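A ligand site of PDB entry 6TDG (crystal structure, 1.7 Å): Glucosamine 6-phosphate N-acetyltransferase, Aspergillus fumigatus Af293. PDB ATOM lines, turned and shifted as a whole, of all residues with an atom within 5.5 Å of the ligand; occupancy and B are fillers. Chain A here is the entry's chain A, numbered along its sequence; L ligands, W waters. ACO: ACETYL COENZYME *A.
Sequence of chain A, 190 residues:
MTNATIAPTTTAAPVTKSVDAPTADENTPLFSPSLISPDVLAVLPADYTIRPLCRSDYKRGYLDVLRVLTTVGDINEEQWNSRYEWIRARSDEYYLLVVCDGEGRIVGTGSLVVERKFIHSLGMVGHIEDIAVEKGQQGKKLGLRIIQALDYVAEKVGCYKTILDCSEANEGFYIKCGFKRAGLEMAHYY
N4P of the ligand is in hydrogen-bond range of O of Ile 131. The backbone NH of Gly 143 is in hydrogen-bond range of an oxygen (O5A) of the ligand (2.9 Å). O5P of the ligand lies close to OD1 of Asn 170, at 3.1 Å. A sulfur (S1P) of the ligand lies close to the side-chain hydroxyl (OH) of Tyr 174 (3.2 Å). O4A of the ligand sits at hydrogen-bond distance from N of Gly 139, at 3.1 Å. The backbone NH of Lys 141 lies within hydrogen-bond range of an oxygen (O1A) of the ligand (2.8 Å). NZ of Lys 141 is in salt-bridge range of O9A of the ligand, at 3.2 Å. The backbone carbonyl oxygen (O) of Ala 169 is in hydrogen-bond range of a nitrogen (N6A) of the ligand, at 3.1 Å. O1A of the ligand is in hydrogen-bond range of N of Lys 140 (3.4 Å). N of Ile 131 sits at hydrogen-bond distance from O of the ligand (3.0 Å). The backbone NH (N) of Val 133 sits at hydrogen-bond distance from an oxygen (O9P) of the ligand (3.1 Å). The side-chain amino group (NZ) of Lys 176 is in salt-bridge range of an oxygen (O8A) of the ligand, 2.7 Å away. The backbone NH (N) of Asp 130 lies within hydrogen-bond range of an oxygen (O) of the ligand (3.4 Å). The backbone NH of Leu 144 is in hydrogen-bond range of an oxygen (O2A) of the ligand (2.8 Å). The side-chain amide oxygen (OE1) of Gln 138 lies close to an oxygen (OAP) of the ligand (3.4 Å).
O of Val 133 lies within hydrogen-bond range of NE2 of Gln 138. O of Phe 173 sits at hydrogen-bond distance from SG of Cys 177 (3.4 Å).
Residues that only touch the ligand: Val 68, Leu 69, Ile 128, Ala 132, Leu 142, Asp 165, Gly 172 and Phe 173. Hydrophobic or aromatic side chains within 4 Å of the ligand: Val 68, Leu 69, Ile 131, Val 133, Leu 144, Phe 173 and Tyr 174. 21 residues have an atom within 4 Å of the ligand: Val 68, Leu 69, Ile 128, Asp 130, Ile 131, Ala 132, Val 133, Gln 138, Gly 139, Lys 140, Lys 141, Leu 142, Gly 143, Leu 144, Asp 165, Ala 169, Asn 170, Gly 172, Phe 173, Tyr 174 and Lys 176.
Water W4 lies within hydrogen-bond range of an oxygen (O1A) of the ligand (2.5 Å) and the backbone carbonyl oxygen of Gly 139 (2.9 Å). Water W1 lies within hydrogen-bond range of an oxygen (O4A) of the ligand (2.7 Å) and the backbone NH (N) of Gly 139 (3.4 Å). Water W5 bridges N3A of the ligand and NZ of Lys 176. Water W6 lies within hydrogen-bond range of a nitrogen (N1A) of the ligand (2.8 Å), the backbone carbonyl oxygen of Ala 169 (3.0 Å) and the backbone NH of Gly 172 (3.1 Å). Water W7 bridges the side-chain amide oxygen (OD1) of Asn 170 (3.0 Å) and a sulfur (S1P) of the ligand (3.4 Å). Water W3 lies within hydrogen-bond range of the backbone NH (N) of Asp 130 (2.9 Å), the side-chain carboxylate (OE1) of Glu 129 (3.0 Å) and an oxygen (O) of the ligand (3.5 Å).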
ATOM      1  N   VAL A  68       5.064 -29.185  -9.933  1.00  0.00           N
ATOM      2  CA  VAL A  68       5.748 -28.330  -8.912  1.00  0.00           C
ATOM      3  C   VAL A  68       6.737 -29.184  -8.110  1.00  0.00           C
ATOM      4  O   VAL A  68       7.606 -28.579  -7.437  1.00  0.00           O
ATOM      5  CB  VAL A  68       4.752 -27.591  -8.006  1.00  0.00           C
ATOM      6  CG1 VAL A  68       3.711 -26.879  -8.867  1.00  0.00           C
ATOM      7  CG2 VAL A  68       4.101 -28.525  -7.012  1.00  0.00           C
ATOM      8  N   LEU A  69       6.553 -30.495  -8.100  1.00  0.00           N
ATOM      9  CA  LEU A  69       7.336 -31.424  -7.228  1.00  0.00           C
ATOM     10  C   LEU A  69       8.703 -31.633  -7.843  1.00  0.00           C
ATOM     11  O   LEU A  69       9.725 -31.408  -7.182  1.00  0.00           O
ATOM     12  CB  LEU A  69       6.640 -32.779  -7.154  1.00  0.00           C
ATOM     13  CG  LEU A  69       5.817 -32.992  -5.903  1.00  0.00           C
ATOM     14  CD1 LEU A  69       5.106 -34.348  -5.947  1.00  0.00           C
ATOM     15  CD2 LEU A  69       6.707 -32.846  -4.668  1.00  0.00           C
ATOM     16  N   ILE A 128       3.367 -40.538   3.730  1.00  0.00           N
ATOM     17  CA  ILE A 128       2.828 -39.367   3.020  1.00  0.00           C
ATOM     18  C   ILE A 128       3.769 -39.051   1.861  1.00  0.00           C
ATOM     19  O   ILE A 128       5.040 -38.929   2.089  1.00  0.00           O
ATOM     20  CB  ILE A 128       2.618 -38.227   3.998  1.00  0.00           C
ATOM     21  CG1 ILE A 128       1.345 -38.442   4.802  1.00  0.00           C
ATOM     22  CG2 ILE A 128       2.619 -36.904   3.257  1.00  0.00           C
ATOM     23  CD1 ILE A 128       1.040 -37.297   5.655  1.00  0.00           C
ATOM     24  N   GLU A 129       3.235 -38.942   0.670  1.00  0.00           N
ATOM     25  CA  GLU A 129       4.048 -38.786  -0.549  1.00  0.00           C
ATOM     26  C   GLU A 129       3.432 -37.763  -1.507  1.00  0.00           C
ATOM     27  O   GLU A 129       2.178 -37.616  -1.557  1.00  0.00           O
ATOM     28  CB  GLU A 129       4.214 -40.104  -1.311  1.00  0.00           C
ATOM     29  CG  GLU A 129       4.753 -41.222  -0.447  1.00  0.00           C
ATOM     30  CD  GLU A 129       6.250 -41.160  -0.210  1.00  0.00           C
ATOM     31  OE1 GLU A 129       6.934 -40.495  -1.014  1.00  0.00           O
ATOM     32  OE2 GLU A 129       6.718 -41.767   0.817  1.00  0.00           O
ATOM     33  N   ASP A 130       4.322 -37.163  -2.288  1.00  0.00           N
ATOM     34  CA  ASP A 130       3.932 -36.455  -3.537  1.00  0.00           C
ATOM     35  C   ASP A 130       2.881 -35.405  -3.180  1.00  0.00           C
ATOM     36  O   ASP A 130       1.819 -35.271  -3.896  1.00  0.00           O
ATOM     37  CB  ASP A 130       3.494 -37.470  -4.573  1.00  0.00           C
ATOM     38  CG  ASP A 130       4.608 -38.441  -4.981  1.00  0.00           C
ATOM     39  OD1 ASP A 130       5.778 -38.076  -4.844  1.00  0.00           O
ATOM     40  OD2 ASP A 130       4.269 -39.535  -5.435  1.00  0.00           O
ATOM     41  N   ILE A 131       3.235 -34.570  -2.218  1.00  0.00           N
ATOM     42  CA  ILE A 131       2.394 -33.405  -1.762  1.00  0.00           C
ATOM     43  C   ILE A 131       2.723 -32.218  -2.672  1.00  0.00           C
ATOM     44  O   ILE A 131       3.906 -31.798  -2.757  1.00  0.00           O
ATOM     45  CB  ILE A 131       2.627 -33.051  -0.296  1.00  0.00           C
ATOM     46  CG1 ILE A 131       2.424 -34.264   0.607  1.00  0.00           C
ATOM     47  CG2 ILE A 131       1.756 -31.883   0.155  1.00  0.00           C
ATOM     48  CD1 ILE A 131       1.060 -34.930   0.488  1.00  0.00           C
ATOM     49  N   ALA A 132       1.722 -31.634  -3.332  1.00  0.00           N
ATOM     50  CA  ALA A 132       1.959 -30.586  -4.343  1.00  0.00           C
ATOM     51  C   ALA A 132       0.747 -29.649  -4.347  1.00  0.00           C
ATOM     52  O   ALA A 132      -0.373 -30.186  -4.348  1.00  0.00           O
ATOM     53  CB  ALA A 132       2.138 -31.173  -5.679  1.00  0.00           C
ATOM     54  N   VAL A 133       0.991 -28.341  -4.305  1.00  0.00           N
ATOM     55  CA  VAL A 133      -0.036 -27.294  -4.517  1.00  0.00           C
ATOM     56  C   VAL A 133       0.455 -26.398  -5.658  1.00  0.00           C
ATOM     57  O   VAL A 133       1.634 -25.947  -5.596  1.00  0.00           O
ATOM     58  CB  VAL A 133      -0.250 -26.469  -3.249  1.00  0.00           C
ATOM     59  CG1 VAL A 133      -1.167 -25.276  -3.517  1.00  0.00           C
ATOM     60  CG2 VAL A 133      -0.704 -27.310  -2.081  1.00  0.00           C
ATOM     61  N   GLN A 137      -1.663 -21.099  -5.979  1.00  0.00           N
ATOM     62  CA  GLN A 137      -2.572 -21.507  -4.893  1.00  0.00           C
ATOM     63  C   GLN A 137      -1.810 -21.793  -3.593  1.00  0.00           C
ATOM     64  O   GLN A 137      -2.432 -22.147  -2.598  1.00  0.00           O
ATOM     65  CB  GLN A 137      -3.424 -22.707  -5.310  1.00  0.00           C
ATOM     66  CG  GLN A 137      -4.293 -22.399  -6.530  1.00  0.00           C
ATOM     67  CD  GLN A 137      -5.496 -21.593  -6.139  1.00  0.00           C
ATOM     68  OE1 GLN A 137      -6.084 -21.783  -5.089  1.00  0.00           O
ATOM     69  NE2 GLN A 137      -5.772 -20.576  -6.942  1.00  0.00           N
ATOM     70  N   GLN A 138      -0.490 -21.599  -3.567  1.00  0.00           N
ATOM     71  CA  GLN A 138       0.308 -21.876  -2.360  1.00  0.00           C
ATOM     72  C   GLN A 138       0.100 -20.771  -1.332  1.00  0.00           C
ATOM     73  O   GLN A 138      -0.423 -19.701  -1.679  1.00  0.00           O
ATOM     74  CB  GLN A 138       1.778 -22.059  -2.745  1.00  0.00           C
ATOM     75  CG  GLN A 138       2.074 -23.364  -3.441  1.00  0.00           C
ATOM     76  CD  GLN A 138       3.521 -23.460  -3.853  1.00  0.00           C
ATOM     77  OE1 GLN A 138       4.335 -22.643  -3.414  1.00  0.00           O
ATOM     78  NE2 GLN A 138       3.818 -24.424  -4.709  1.00  0.00           N
ATOM     79  N   GLY A 139       0.408 -21.057  -0.076  1.00  0.00           N
ATOM     80  CA  GLY A 139       0.320 -20.096   1.031  1.00  0.00           C
ATOM     81  C   GLY A 139      -1.084 -19.724   1.459  1.00  0.00           C
ATOM     82  O   GLY A 139      -1.222 -18.718   2.200  1.00  0.00           O
ATOM     83  N   LYS A 140      -2.066 -20.591   1.184  1.00  0.00           N
ATOM     84  CA  LYS A 140      -3.468 -20.442   1.659  1.00  0.00           C
ATOM     85  C   LYS A 140      -3.921 -21.654   2.466  1.00  0.00           C
ATOM     86  O   LYS A 140      -5.126 -21.875   2.474  1.00  0.00           O
ATOM     87  CB  LYS A 140      -4.464 -20.389   0.498  1.00  0.00           C
ATOM     88  CG  LYS A 140      -4.088 -19.568  -0.712  1.00  0.00           C
ATOM     89  CD  LYS A 140      -4.942 -19.980  -1.930  1.00  0.00           C
ATOM     90  CE  LYS A 140      -5.621 -18.835  -2.649  1.00  0.00           C
ATOM     91  NZ  LYS A 140      -4.643 -18.013  -3.402  1.00  0.00           N
ATOM     92  N   LYS A 141      -3.000 -22.436   3.050  1.00  0.00           N
ATOM     93  CA  LYS A 141      -3.300 -23.581   3.950  1.00  0.00           C
ATOM     94  C   LYS A 141      -3.767 -24.811   3.163  1.00  0.00           C
ATOM     95  O   LYS A 141      -4.207 -25.748   3.844  1.00  0.00           O
ATOM     96  CB  LYS A 141      -4.340 -23.231   5.010  1.00  0.00           C
ATOM     97  CG  LYS A 141      -4.051 -21.964   5.798  1.00  0.00           C
ATOM     98  CD  LYS A 141      -3.078 -22.146   6.932  1.00  0.00           C
ATOM     99  CE  LYS A 141      -3.032 -20.986   7.917  1.00  0.00           C
ATOM    100  NZ  LYS A 141      -2.902 -19.703   7.183  1.00  0.00           N
ATOM    101  N   LEU A 142      -3.707 -24.830   1.836  1.00  0.00           N
ATOM    102  CA  LEU A 142      -4.150 -26.024   1.075  1.00  0.00           C
ATOM    103  C   LEU A 142      -3.197 -27.198   1.379  1.00  0.00           C
ATOM    104  O   LEU A 142      -3.724 -28.303   1.597  1.00  0.00           O
ATOM    105  CB  LEU A 142      -4.235 -25.741  -0.416  1.00  0.00           C
ATOM    106  CG  LEU A 142      -5.269 -24.679  -0.828  1.00  0.00           C
ATOM    107  CD1 LEU A 142      -5.271 -24.564  -2.335  1.00  0.00           C
ATOM    108  CD2 LEU A 142      -6.663 -24.987  -0.242  1.00  0.00           C
ATOM    109  N   GLY A 143      -1.876 -27.003   1.446  1.00  0.00           N
ATOM    110  CA  GLY A 143      -0.966 -28.096   1.856  1.00  0.00           C
ATOM    111  C   GLY A 143      -1.302 -28.608   3.246  1.00  0.00           C
ATOM    112  O   GLY A 143      -1.337 -29.835   3.447  1.00  0.00           O
ATOM    113  N   LEU A 144      -1.515 -27.730   4.197  1.00  0.00           N
ATOM    114  CA  LEU A 144      -1.935 -28.130   5.568  1.00  0.00           C
ATOM    115  C   LEU A 144      -3.185 -29.005   5.473  1.00  0.00           C
ATOM    116  O   LEU A 144      -3.204 -29.999   6.194  1.00  0.00           O
ATOM    117  CB  LEU A 144      -2.178 -26.908   6.449  1.00  0.00           C
ATOM    118  CG  LEU A 144      -2.772 -27.164   7.818  1.00  0.00           C
ATOM    119  CD1 LEU A 144      -1.813 -27.928   8.718  1.00  0.00           C
ATOM    120  CD2 LEU A 144      -3.142 -25.866   8.470  1.00  0.00           C
ATOM    121  N   ARG A 145      -4.201 -28.584   4.728  1.00  0.00           N
ATOM    122  CA  ARG A 145      -5.460 -29.355   4.632  1.00  0.00           C
ATOM    123  C   ARG A 145      -5.168 -30.740   4.015  1.00  0.00           C
ATOM    124  O   ARG A 145      -5.747 -31.735   4.498  1.00  0.00           O
ATOM    125  CB  ARG A 145      -6.527 -28.591   3.847  1.00  0.00           C
ATOM    126  CG  ARG A 145      -6.869 -27.203   4.370  1.00  0.00           C
ATOM    127  CD  ARG A 145      -7.011 -27.144   5.856  1.00  0.00           C
ATOM    128  NE  ARG A 145      -7.209 -25.800   6.392  1.00  0.00           N
ATOM    129  CZ  ARG A 145      -7.122 -25.496   7.683  1.00  0.00           C
ATOM    130  NH1 ARG A 145      -6.813 -26.418   8.575  1.00  0.00           N
ATOM    131  NH2 ARG A 145      -7.354 -24.260   8.079  1.00  0.00           N
ATOM    132  N   LEU A 164       7.115 -39.288   6.639  1.00  0.00           N
ATOM    133  CA  LEU A 164       7.412 -38.730   5.310  1.00  0.00           C
ATOM    134  C   LEU A 164       8.857 -38.280   5.372  1.00  0.00           C
ATOM    135  O   LEU A 164       9.378 -38.103   6.507  1.00  0.00           O
ATOM    136  CB  LEU A 164       6.454 -37.568   5.009  1.00  0.00           C
ATOM    137  CG  LEU A 164       6.458 -36.382   5.971  1.00  0.00           C
ATOM    138  CD1 LEU A 164       7.506 -35.303   5.641  1.00  0.00           C
ATOM    139  CD2 LEU A 164       5.089 -35.746   6.020  1.00  0.00           C
ATOM    140  N   ASP A 165       9.428 -38.073   4.206  1.00  0.00           N
ATOM    141  CA  ASP A 165      10.751 -37.444   4.020  1.00  0.00           C
ATOM    142  C   ASP A 165      10.535 -36.043   3.444  1.00  0.00           C
ATOM    143  O   ASP A 165       9.687 -35.884   2.533  1.00  0.00           O
ATOM    144  CB  ASP A 165      11.584 -38.320   3.120  1.00  0.00           C
ATOM    145  CG  ASP A 165      11.910 -39.696   3.681  1.00  0.00           C
ATOM    146  OD1 ASP A 165      12.262 -39.792   4.867  1.00  0.00           O
ATOM    147  OD2 ASP A 165      11.863 -40.633   2.904  1.00  0.00           O
ATOM    148  N   CYS A 166      11.328 -35.091   3.898  1.00  0.00           N
ATOM    149  CA  CYS A 166      11.307 -33.712   3.412  1.00  0.00           C
ATOM    150  C   CYS A 166      12.712 -33.162   3.315  1.00  0.00           C
ATOM    151  O   CYS A 166      13.645 -33.830   3.687  1.00  0.00           O
ATOM    152  CB  CYS A 166      10.428 -32.822   4.292  1.00  0.00           C
ATOM    153  SG  CYS A 166      11.072 -32.513   5.932  1.00  0.00           S
ATOM    154  N   ALA A 169      14.542 -27.298   3.580  1.00  0.00           N
ATOM    155  CA  ALA A 169      13.835 -26.066   3.103  1.00  0.00           C
ATOM    156  C   ALA A 169      12.317 -26.169   3.356  1.00  0.00           C
ATOM    157  O   ALA A 169      11.663 -25.099   3.558  1.00  0.00           O
ATOM    158  CB  ALA A 169      14.095 -25.873   1.625  1.00  0.00           C
ATOM    159  N   ASN A 170      11.744 -27.361   3.400  1.00  0.00           N
ATOM    160  CA  ASN A 170      10.289 -27.412   3.646  1.00  0.00           C
ATOM    161  C   ASN A 170      10.059 -28.119   4.979  1.00  0.00           C
ATOM    162  O   ASN A 170       8.920 -28.310   5.335  1.00  0.00           O
ATOM    163  CB  ASN A 170       9.470 -27.828   2.404  1.00  0.00           C
ATOM    164  CG  ASN A 170       9.746 -29.232   1.934  1.00  0.00           C
ATOM    165  OD1 ASN A 170       9.430 -29.612   0.797  1.00  0.00           O
ATOM    166  ND2 ASN A 170      10.338 -29.998   2.824  1.00  0.00           N
ATOM    167  N   GLU A 171      11.088 -28.323   5.802  1.00  0.00           N
ATOM    168  CA  GLU A 171      10.842 -28.871   7.157  1.00  0.00           C
ATOM    169  C   GLU A 171       9.853 -28.005   7.932  1.00  0.00           C
ATOM    170  O   GLU A 171       9.048 -28.570   8.674  1.00  0.00           O
ATOM    171  CB  GLU A 171      12.162 -29.026   7.938  1.00  0.00           C
ATOM    172  CG  GLU A 171      11.978 -29.703   9.275  1.00  0.00           C
ATOM    173  CD  GLU A 171      13.174 -29.788  10.208  1.00  0.00           C
ATOM    174  OE1 GLU A 171      14.228 -29.241   9.870  1.00  0.00           O
ATOM    175  OE2 GLU A 171      13.018 -30.429  11.263  1.00  0.00           O
ATOM    176  N   GLY A 172       9.904 -26.676   7.789  1.00  0.00           N
ATOM    177  CA  GLY A 172       9.072 -25.730   8.536  1.00  0.00           C
ATOM    178  C   GLY A 172       7.593 -25.919   8.251  1.00  0.00           C
ATOM    179  O   GLY A 172       6.776 -25.759   9.169  1.00  0.00           O
ATOM    180  N   PHE A 173       7.280 -26.307   7.027  1.00  0.00           N
ATOM    181  CA  PHE A 173       5.903 -26.647   6.604  1.00  0.00           C
ATOM    182  C   PHE A 173       5.443 -27.851   7.432  1.00  0.00           C
ATOM    183  O   PHE A 173       4.369 -27.744   7.994  1.00  0.00           O
ATOM    184  CB  PHE A 173       5.843 -26.919   5.108  1.00  0.00           C
ATOM    185  CG  PHE A 173       4.527 -27.509   4.685  1.00  0.00           C
ATOM    186  CD1 PHE A 173       3.346 -26.791   4.846  1.00  0.00           C
ATOM    187  CD2 PHE A 173       4.475 -28.797   4.206  1.00  0.00           C
ATOM    188  CE1 PHE A 173       2.119 -27.360   4.517  1.00  0.00           C
ATOM    189  CE2 PHE A 173       3.265 -29.353   3.831  1.00  0.00           C
ATOM    190  CZ  PHE A 173       2.086 -28.648   4.008  1.00  0.00           C
ATOM    191  N   TYR A 174       6.235 -28.917   7.487  1.00  0.00           N
ATOM    192  CA  TYR A 174       5.848 -30.178   8.197  1.00  0.00           C
ATOM    193  C   TYR A 174       5.768 -29.922   9.694  1.00  0.00           C
ATOM    194  O   TYR A 174       4.851 -30.461  10.306  1.00  0.00           O
ATOM    195  CB  TYR A 174       6.719 -31.341   7.764  1.00  0.00           C
ATOM    196  CG  TYR A 174       6.452 -31.687   6.338  1.00  0.00           C
ATOM    197  CD1 TYR A 174       5.191 -32.137   5.998  1.00  0.00           C
ATOM    198  CD2 TYR A 174       7.327 -31.351   5.317  1.00  0.00           C
ATOM    199  CE1 TYR A 174       4.868 -32.447   4.696  1.00  0.00           C
ATOM    200  CE2 TYR A 174       6.997 -31.624   3.995  1.00  0.00           C
ATOM    201  CZ  TYR A 174       5.743 -32.153   3.692  1.00  0.00           C
ATOM    202  OH  TYR A 174       5.296 -32.392   2.422  1.00  0.00           O
ATOM    203  N   LYS A 176       4.736 -27.061  11.017  1.00  0.00           N
ATOM    204  CA  LYS A 176       3.416 -26.377  11.178  1.00  0.00           C
ATOM    205  C   LYS A 176       2.271 -27.369  10.960  1.00  0.00           C
ATOM    206  O   LYS A 176       1.155 -27.099  11.484  1.00  0.00           O
ATOM    207  CB  LYS A 176       3.360 -25.165  10.246  1.00  0.00           C
ATOM    208  CG  LYS A 176       4.278 -24.015  10.686  1.00  0.00           C
ATOM    209  CD  LYS A 176       3.694 -22.625  10.536  1.00  0.00           C
ATOM    210  CE  LYS A 176       4.547 -21.507  11.121  1.00  0.00           C
ATOM    211  NZ  LYS A 176       4.496 -20.302  10.262  1.00  0.00           N
ATOM    212  N   CYS A 177       2.524 -28.521  10.311  1.00  0.00           N
ATOM    213  CA  CYS A 177       1.508 -29.605  10.202  1.00  0.00           C
ATOM    214  C   CYS A 177       1.525 -30.554  11.411  1.00  0.00           C
ATOM    215  O   CYS A 177       0.771 -31.534  11.407  1.00  0.00           O
ATOM    216  CB  CYS A 177       1.684 -30.385   8.901  1.00  0.00           C
ATOM    217  SG  CYS A 177       1.424 -29.417   7.397  1.00  0.00           S
HETATM  218  N1A ACO L   1       8.848 -23.458   5.143  1.00  0.00           N
HETATM  219  C2A ACO L   1       8.285 -22.938   6.241  1.00  0.00           C
HETATM  220  N3A ACO L   1       6.948 -22.656   6.351  1.00  0.00           N
HETATM  221  C4A ACO L   1       6.158 -23.010   5.277  1.00  0.00           C
HETATM  222  C5A ACO L   1       6.727 -23.601   4.089  1.00  0.00           C
HETATM  223  C6A ACO L   1       8.146 -23.790   4.044  1.00  0.00           C
HETATM  224  N6A ACO L   1       8.711 -24.330   2.926  1.00  0.00           N
HETATM  225  N7A ACO L   1       5.725 -23.778   3.184  1.00  0.00           N
HETATM  226  C8A ACO L   1       4.614 -23.385   3.773  1.00  0.00           C
HETATM  227  N9A ACO L   1       4.887 -22.881   5.000  1.00  0.00           N
HETATM  228  C1B ACO L   1       3.930 -22.399   5.998  1.00  0.00           C
HETATM  229  C2B ACO L   1       2.853 -21.523   5.460  1.00  0.00           C
HETATM  230  O2B ACO L   1       3.233 -20.168   5.369  1.00  0.00           O
HETATM  231  C3B ACO L   1       1.783 -21.746   6.511  1.00  0.00           C
HETATM  232  O3B ACO L   1       2.167 -21.023   7.665  1.00  0.00           O
HETATM  233  P3B ACO L   1       1.023 -20.387   8.712  1.00  0.00           P
HETATM  234  O7A ACO L   1       0.374 -21.553   9.369  1.00  0.00           O
HETATM  235  O8A ACO L   1       1.955 -19.611   9.575  1.00  0.00           O
HETATM  236  O9A ACO L   1       0.224 -19.582   7.722  1.00  0.00           O
HETATM  237  C4B ACO L   1       1.918 -23.217   6.868  1.00  0.00           C
HETATM  238  O4B ACO L   1       3.289 -23.523   6.650  1.00  0.00           O
HETATM  239  C5B ACO L   1       1.005 -24.164   6.094  1.00  0.00           C
HETATM  240  O5B ACO L   1       1.307 -23.966   4.733  1.00  0.00           O
HETATM  241  P1A ACO L   1       0.314 -23.963   3.500  1.00  0.00           P
HETATM  242  O1A ACO L   1      -0.251 -22.588   3.253  1.00  0.00           O
HETATM  243  O2A ACO L   1      -0.677 -25.044   3.818  1.00  0.00           O
HETATM  244  O3A ACO L   1       1.284 -24.319   2.342  1.00  0.00           O
HETATM  245  P2A ACO L   1       1.174 -24.648   0.819  1.00  0.00           P
HETATM  246  O4A ACO L   1       1.999 -23.735   0.041  1.00  0.00           O
HETATM  247  O5A ACO L   1      -0.329 -24.768   0.560  1.00  0.00           O
HETATM  248  O6A ACO L   1       1.768 -26.170   0.799  1.00  0.00           O
HETATM  249  CBP ACO L   1       3.749 -27.206  -0.040  1.00  0.00           C
HETATM  250  CCP ACO L   1       3.121 -26.471   1.139  1.00  0.00           C
HETATM  251  CDP ACO L   1       3.042 -28.489  -0.316  1.00  0.00           C
HETATM  252  CEP ACO L   1       5.231 -27.499   0.307  1.00  0.00           C
HETATM  253  CAP ACO L   1       3.674 -26.351  -1.278  1.00  0.00           C
HETATM  254  OAP ACO L   1       4.302 -25.081  -1.051  1.00  0.00           O
HETATM  255  C9P ACO L   1       4.348 -26.969  -2.444  1.00  0.00           C
HETATM  256  O9P ACO L   1       3.773 -27.695  -3.214  1.00  0.00           O
HETATM  257  N8P ACO L   1       5.666 -26.758  -2.631  1.00  0.00           N
HETATM  258  C7P ACO L   1       6.244 -27.416  -3.732  1.00  0.00           C
HETATM  259  C6P ACO L   1       6.377 -28.922  -3.741  1.00  0.00           C
HETATM  260  C5P ACO L   1       6.902 -29.460  -2.411  1.00  0.00           C
HETATM  261  O5P ACO L   1       7.854 -29.027  -1.769  1.00  0.00           O
HETATM  262  N4P ACO L   1       6.197 -30.483  -1.953  1.00  0.00           N
HETATM  263  C3P ACO L   1       6.539 -31.150  -0.671  1.00  0.00           C
HETATM  264  C2P ACO L   1       7.345 -32.372  -1.036  1.00  0.00           C
HETATM  265  S1P ACO L   1       7.731 -33.266   0.495  1.00  0.00           S
HETATM  266  C   ACO L   1       6.538 -34.464   0.376  1.00  0.00           C
HETATM  267  O   ACO L   1       5.727 -34.543  -0.562  1.00  0.00           O
HETATM  268  CH3 ACO L   1       6.468 -35.440   1.497  1.00  0.00           C
HETATM  269  O   HOH W   1       3.530 -21.755   0.945  1.00  0.00           O
HETATM  270  O   HOH W   2      -2.217 -23.004   0.004  1.00  0.00           O
HETATM  271  O   HOH W   3       7.133 -37.563  -1.576  1.00  0.00           O
HETATM  272  O   HOH W   4      -0.235 -20.353   4.360  1.00  0.00           O
HETATM  273  O   HOH W   5       6.870 -21.399   8.877  1.00  0.00           O
HETATM  274  O   HOH W   6      11.275 -24.198   6.427  1.00  0.00           O
HETATM  275  O   HOH W   7      10.878 -32.069  -0.045  1.00  0.00           O
HETATM  276  O   HOH W   8       6.702 -24.525  -5.465  1.00  0.00           O
HETATM  277  O   HOH W   9       6.355 -23.927   0.492  1.00  0.00           O
